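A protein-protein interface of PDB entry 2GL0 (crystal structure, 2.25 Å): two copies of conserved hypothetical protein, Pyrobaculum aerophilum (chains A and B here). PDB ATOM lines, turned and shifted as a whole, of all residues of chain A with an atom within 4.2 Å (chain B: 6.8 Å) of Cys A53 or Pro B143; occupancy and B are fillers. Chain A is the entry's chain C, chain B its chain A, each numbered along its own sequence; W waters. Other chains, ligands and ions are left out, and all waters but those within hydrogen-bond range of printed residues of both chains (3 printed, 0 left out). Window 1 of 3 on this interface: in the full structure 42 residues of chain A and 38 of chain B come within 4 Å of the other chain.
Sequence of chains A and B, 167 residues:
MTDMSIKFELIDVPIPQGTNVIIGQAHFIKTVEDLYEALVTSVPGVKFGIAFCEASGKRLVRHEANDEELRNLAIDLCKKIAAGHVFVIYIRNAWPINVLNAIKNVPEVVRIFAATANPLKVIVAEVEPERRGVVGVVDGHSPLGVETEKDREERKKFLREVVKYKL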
ATOM      1  N   PHE A  52       5.944 -31.432 -21.303  1.00  0.00           N
ATOM      2  CA  PHE A  52       6.089 -30.367 -20.374  1.00  0.00           C
ATOM      3  C   PHE A  52       4.823 -30.310 -19.537  1.00  0.00           C
ATOM      4  O   PHE A  52       3.724 -30.505 -20.048  1.00  0.00           O
ATOM      5  CB  PHE A  52       6.389 -29.078 -21.167  1.00  0.00           C
ATOM      6  CG  PHE A  52       6.310 -27.777 -20.375  1.00  0.00           C
ATOM      7  CD1 PHE A  52       7.299 -27.451 -19.401  1.00  0.00           C
ATOM      8  CD2 PHE A  52       5.338 -26.808 -20.694  1.00  0.00           C
ATOM      9  CE1 PHE A  52       7.260 -26.290 -18.719  1.00  0.00           C
ATOM     10  CE2 PHE A  52       5.336 -25.623 -19.995  1.00  0.00           C
ATOM     11  CZ  PHE A  52       6.301 -25.375 -18.994  1.00  0.00           C
ATOM     12  N   CYS A  53       4.963 -30.037 -18.250  1.00  0.00           N
ATOM     13  CA  CYS A  53       3.802 -29.979 -17.363  1.00  0.00           C
ATOM     14  C   CYS A  53       3.415 -28.549 -17.253  1.00  0.00           C
ATOM     15  O   CYS A  53       3.941 -27.870 -16.390  1.00  0.00           O
ATOM     16  CB  CYS A  53       4.123 -30.481 -15.947  1.00  0.00           C
ATOM     17  SG  CYS A  53       4.432 -32.206 -15.847  1.00  0.00           S
ATOM     18  N   GLU A  54       2.490 -28.106 -18.134  1.00  0.00           N
ATOM     19  CA  GLU A  54       1.791 -26.831 -17.939  1.00  0.00           C
ATOM     20  C   GLU A  54       1.172 -26.676 -16.513  1.00  0.00           C
ATOM     21  O   GLU A  54       0.402 -27.478 -16.077  1.00  0.00           O
ATOM     22  CB  GLU A  54       0.789 -26.638 -19.060  1.00  0.00           C
ATOM     23  CG  GLU A  54       0.138 -25.287 -19.108  1.00  0.00           C
ATOM     24  CD  GLU A  54      -1.146 -25.306 -19.931  1.00  0.00           C
ATOM     25  OE1 GLU A  54      -1.721 -26.414 -20.237  1.00  0.00           O
ATOM     26  OE2 GLU A  54      -1.570 -24.179 -20.274  1.00  0.00           O
ATOM     27  N   ALA A  55       1.555 -25.650 -15.783  1.00  0.00           N
ATOM     28  CA  ALA A  55       1.340 -25.590 -14.342  1.00  0.00           C
ATOM     29  C   ALA A  55       0.184 -24.688 -13.974  1.00  0.00           C
ATOM     30  O   ALA A  55      -0.174 -24.540 -12.786  1.00  0.00           O
ATOM     31  CB  ALA A  55       2.656 -25.085 -13.650  1.00  0.00           C
ATOM     32  N   ARG A  59      -3.684 -26.550 -17.469  1.00  0.00           N
ATOM     33  CA  ARG A  59      -2.742 -27.474 -16.804  1.00  0.00           C
ATOM     34  C   ARG A  59      -2.527 -28.809 -17.524  1.00  0.00           C
ATOM     35  O   ARG A  59      -2.650 -29.864 -16.924  1.00  0.00           O
ATOM     36  CB  ARG A  59      -3.173 -27.709 -15.370  1.00  0.00           C
ATOM     37  CG  ARG A  59      -2.987 -26.540 -14.477  1.00  0.00           C
ATOM     38  CD  ARG A  59      -3.975 -26.585 -13.348  1.00  0.00           C
ATOM     39  NE  ARG A  59      -3.896 -27.842 -12.613  1.00  0.00           N
ATOM     40  CZ  ARG A  59      -4.639 -28.133 -11.554  1.00  0.00           C
ATOM     41  NH1 ARG A  59      -5.540 -27.263 -11.101  1.00  0.00           N
ATOM     42  NH2 ARG A  59      -4.476 -29.284 -10.950  1.00  0.00           N
ATOM     43  N   VAL A  61      -0.356 -31.853 -19.901  1.00  0.00           N
ATOM     44  CA  VAL A  61       0.956 -32.327 -20.410  1.00  0.00           C
ATOM     45  C   VAL A  61       1.036 -31.993 -21.875  1.00  0.00           C
ATOM     46  O   VAL A  61       0.281 -32.555 -22.632  1.00  0.00           O
ATOM     47  CB  VAL A  61       1.254 -33.895 -20.149  1.00  0.00           C
ATOM     48  CG1 VAL A  61       2.613 -34.312 -20.693  1.00  0.00           C
ATOM     49  CG2 VAL A  61       1.263 -34.227 -18.645  1.00  0.00           C
ATOM     50  N   CYS A  78       6.011 -37.590 -17.090  1.00  0.00           N
ATOM     51  CA  CYS A  78       5.376 -36.367 -16.590  1.00  0.00           C
ATOM     52  C   CYS A  78       4.203 -36.644 -15.671  1.00  0.00           C
ATOM     53  O   CYS A  78       4.005 -35.932 -14.698  1.00  0.00           O
ATOM     54  CB  CYS A  78       4.965 -35.415 -17.713  1.00  0.00           C
ATOM     55  SG  CYS A  78       6.420 -34.533 -18.391  1.00  0.00           S
ATOM     56  N   ALA A  82       4.286 -35.507 -11.881  1.00  0.00           N
ATOM     57  CA  ALA A  82       3.103 -34.645 -11.724  1.00  0.00           C
ATOM     58  C   ALA A  82       3.483 -33.401 -10.955  1.00  0.00           C
ATOM     59  O   ALA A  82       2.863 -33.053  -9.934  1.00  0.00           O
ATOM     60  CB  ALA A  82       1.885 -35.420 -11.074  1.00  0.00           C
ATOM     61  N   ALA A  83       4.471 -32.668 -11.462  1.00  0.00           N
ATOM     62  CA  ALA A  83       4.900 -31.475 -10.737  1.00  0.00           C
ATOM     63  C   ALA A  83       4.974 -30.368 -11.690  1.00  0.00           C
ATOM     64  O   ALA A  83       5.670 -30.521 -12.713  1.00  0.00           O
ATOM     65  CB  ALA A  83       6.253 -31.681 -10.120  1.00  0.00           C
ATOM     66  N   GLY A  84       4.354 -29.239 -11.334  1.00  0.00           N
ATOM     67  CA  GLY A  84       4.333 -28.032 -12.173  1.00  0.00           C
ATOM     68  C   GLY A  84       5.703 -27.613 -12.729  1.00  0.00           C
ATOM     69  O   GLY A  84       6.643 -27.418 -11.956  1.00  0.00           O
ATOM     70  N   HIS A  85       5.793 -27.553 -14.072  1.00  0.00           N
ATOM     71  CA  HIS A  85       6.874 -26.930 -14.851  1.00  0.00           C
ATOM     72  C   HIS A  85       8.042 -27.795 -15.130  1.00  0.00           C
ATOM     73  O   HIS A  85       9.074 -27.347 -15.618  1.00  0.00           O
ATOM     74  CB  HIS A  85       7.336 -25.646 -14.184  1.00  0.00           C
ATOM     75  CG  HIS A  85       6.562 -24.463 -14.619  1.00  0.00           C
ATOM     76  ND1 HIS A  85       6.734 -23.209 -14.069  1.00  0.00           N
ATOM     77  CD2 HIS A  85       5.575 -24.344 -15.536  1.00  0.00           C
ATOM     78  CE1 HIS A  85       5.908 -22.368 -14.663  1.00  0.00           C
ATOM     79  NE2 HIS A  85       5.216 -23.022 -15.569  1.00  0.00           N
ATOM     80  N   VAL A  86       7.878 -29.045 -14.810  1.00  0.00           N
ATOM     81  CA  VAL A  86       8.873 -30.063 -15.027  1.00  0.00           C
ATOM     82  C   VAL A  86       8.738 -30.572 -16.484  1.00  0.00           C
ATOM     83  O   VAL A  86       7.624 -30.691 -17.062  1.00  0.00           O
ATOM     84  CB  VAL A  86       8.729 -31.143 -13.896  1.00  0.00           C
ATOM     85  CG1 VAL A  86       9.499 -32.381 -14.179  1.00  0.00           C
ATOM     86  CG2 VAL A  86       9.209 -30.547 -12.502  1.00  0.00           C
ATOM     87  N   ASP B 139       6.037 -25.160  -8.026  1.00  0.00           N
ATOM     88  CA  ASP B 139       5.672 -24.149  -8.964  1.00  0.00           C
ATOM     89  C   ASP B 139       4.265 -24.382  -9.644  1.00  0.00           C
ATOM     90  O   ASP B 139       4.073 -25.296 -10.484  1.00  0.00           O
ATOM     91  CB  ASP B 139       6.852 -24.017  -9.969  1.00  0.00           C
ATOM     92  CG  ASP B 139       6.665 -22.898 -10.956  1.00  0.00           C
ATOM     93  OD1 ASP B 139       5.591 -22.231 -10.957  1.00  0.00           O
ATOM     94  OD2 ASP B 139       7.596 -22.644 -11.746  1.00  0.00           O
ATOM     95  N   HIS B 141       0.376 -25.823 -10.316  1.00  0.00           N
ATOM     96  CA  HIS B 141      -0.388 -27.107 -10.001  1.00  0.00           C
ATOM     97  C   HIS B 141      -0.053 -28.298 -10.893  1.00  0.00           C
ATOM     98  O   HIS B 141       0.411 -28.132 -12.002  1.00  0.00           O
ATOM     99  CB  HIS B 141      -1.939 -26.882  -9.966  1.00  0.00           C
ATOM    100  CG  HIS B 141      -2.392 -25.918  -8.887  1.00  0.00           C
ATOM    101  ND1 HIS B 141      -1.848 -24.653  -8.736  1.00  0.00           N
ATOM    102  CD2 HIS B 141      -3.268 -26.070  -7.861  1.00  0.00           C
ATOM    103  CE1 HIS B 141      -2.396 -24.056  -7.694  1.00  0.00           C
ATOM    104  NE2 HIS B 141      -3.258 -24.893  -7.143  1.00  0.00           N
ATOM    105  N   SER B 142      -0.209 -29.501 -10.377  1.00  0.00           N
ATOM    106  CA  SER B 142       0.076 -30.703 -11.120  1.00  0.00           C
ATOM    107  C   SER B 142      -0.913 -30.876 -12.330  1.00  0.00           C
ATOM    108  O   SER B 142      -1.958 -30.211 -12.369  1.00  0.00           O
ATOM    109  CB  SER B 142      -0.011 -31.874 -10.145  1.00  0.00           C
ATOM    110  OG  SER B 142      -1.340 -31.972  -9.698  1.00  0.00           O
ATOM    111  N   PRO B 143      -0.602 -31.763 -13.311  1.00  0.00           N
ATOM    112  CA  PRO B 143      -1.435 -31.817 -14.535  1.00  0.00           C
ATOM    113  C   PRO B 143      -2.910 -32.221 -14.341  1.00  0.00           C
ATOM    114  O   PRO B 143      -3.206 -33.073 -13.497  1.00  0.00           O
ATOM    115  CB  PRO B 143      -0.723 -32.879 -15.393  1.00  0.00           C
ATOM    116  CG  PRO B 143       0.638 -32.920 -14.856  1.00  0.00           C
ATOM    117  CD  PRO B 143       0.497 -32.734 -13.398  1.00  0.00           C
ATOM    118  N   LEU B 144      -3.808 -31.617 -15.132  1.00  0.00           N
ATOM    119  CA  LEU B 144      -5.195 -32.061 -15.179  1.00  0.00           C
ATOM    120  C   LEU B 144      -5.422 -33.123 -16.241  1.00  0.00           C
ATOM    121  O   LEU B 144      -6.343 -33.891 -16.154  1.00  0.00           O
ATOM    122  CB  LEU B 144      -6.134 -30.895 -15.381  1.00  0.00           C
ATOM    123  CG  LEU B 144      -6.337 -29.996 -14.179  1.00  0.00           C
ATOM    124  CD1 LEU B 144      -7.235 -28.837 -14.642  1.00  0.00           C
ATOM    125  CD2 LEU B 144      -6.973 -30.827 -13.031  1.00  0.00           C
ATOM    126  N   GLY B 145      -4.552 -33.188 -17.233  1.00  0.00           N
ATOM    127  CA  GLY B 145      -4.519 -34.346 -18.078  1.00  0.00           C
ATOM    128  C   GLY B 145      -3.491 -34.009 -19.131  1.00  0.00           C
ATOM    129  O   GLY B 145      -2.618 -33.153 -18.888  1.00  0.00           O
ATOM    130  N   VAL B 146      -3.652 -34.666 -20.294  1.00  0.00           N
ATOM    131  CA  VAL B 146      -2.667 -34.721 -21.365  1.00  0.00           C
ATOM    132  C   VAL B 146      -3.182 -33.980 -22.571  1.00  0.00           C
ATOM    133  O   VAL B 146      -4.318 -34.117 -22.896  1.00  0.00           O
ATOM    134  CB  VAL B 146      -2.374 -36.188 -21.710  1.00  0.00           C
ATOM    135  CG1 VAL B 146      -1.527 -36.302 -22.996  1.00  0.00           C
ATOM    136  CG2 VAL B 146      -1.676 -36.877 -20.456  1.00  0.00           C
HETATM  137  O   HOH W   1       1.494 -29.754 -14.111  1.00  0.00           O
HETATM  138  O   HOH W   2       7.086 -27.883  -9.493  1.00  0.00           O
HETATM  139  O   HOH W   3      -1.247 -22.869 -10.980  1.00  0.00           O
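Water W2 lies within hydrogen-bond range of O of Gly A84 (2.5 Å) and N of Asp B139 (3.3 Å). Water W3 lies within hydrogen-bond range of the backbone carbonyl oxygen of Ala A55 and a ring nitrogen (ND1) of His B141. Water W1 lies within hydrogen-bond range of the backbone carbonyl oxygen (O) of His B141 and the backbone carbonyl oxygen (O) of Glu A54.
ND1 of His A85 sits at hydrogen-bond distance from OD2 of Asp B139, 2.5 Å away. The backbone NH (N) of His B141 is in hydrogen-bond range of the backbone carbonyl oxygen (O) of Ala A55. The backbone carbonyl oxygen (O) of Ser B142 lies within hydrogen-bond range of the guanidinium group (NH2) of Arg A59, at 3.0 Å. The backbone NH of Leu B144 is in hydrogen-bond range of the backbone carbonyl oxygen of Arg A59 (2.8 Å). The backbone carbonyl oxygen (O) of Gly B145 is in hydrogen-bond range of the backbone NH (N) of Val A61 (2.8 Å).
Phe A52 touches none of the printed residues of chain B. Printed residues of chain B within 4 Å of Cys A53: Pro B143. Of the printed residues of chain B, Ala A82 touches Ser B142 and Pro B143. Ala A83 touches none of the printed residues of chain B. Of the printed residues of chain A, Pro B143 touches Cys A53 (3.99 Å), Arg A59 (3.3 Å) and Ala A82 (3.6 Å). Of the printed residues of chain A, Leu B144 touches Arg A59 (2.8 Å). Printed residues of chain A within 4 Å of Val B146: Val A61.
Hydrophobic or aromatic side chains of chain A that line the printed part of chain B: Ala A55, Ala A82 and His A85. Of the 7 printed residues of chain B, 7 touch a printed residue of chain A. Hydrophobic or aromatic side chains of chain B that line the printed part of chain A: His B141, Pro B143 and Leu B144. Among the printed residues, 15 pairs touch across the chains.
SG of Cys A53 touches CG of Pro B143, at 3.99 Å. Ala A55 touches Asp B139 (CB to O, 3.5 Å). Arg A59 touches His B141 (CZ to CB, 3.4 Å). Pro B143 touches Arg A59 (CA to O, 3.3 Å). O of Arg A59 touches O of Gly B145, at 3.8 Å. Val A61 touches Val B146 (O to C, 3.7 Å). Ser B142 touches Ala A82 (CB to O, 3.1 Å). CA of Ala A82 touches CD of Pro B143 (3.6 Å). Gly A84 touches Asp B139 (CA to O, 3.2 Å). O of His B141 touches CA of Gly A84 (3.9 Å).
No position is printed for both chains.
The backbone carbonyl oxygen (O) of Ala A83 sits close to the side-chain sulfur (SG) of Cys A53 (3.8 Å). O of Cys A53 is in hydrogen-bond range of N of His A85 (3.0 Å). The backbone NH (N) of Cys A53 is in hydrogen-bond range of the backbone carbonyl oxygen (O) of Val A86, at 3.0 Å. The side-chain carboxylate of Glu A54 sits at hydrogen-bond distance from the backbone NH of Arg A59 (3.4 Å).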
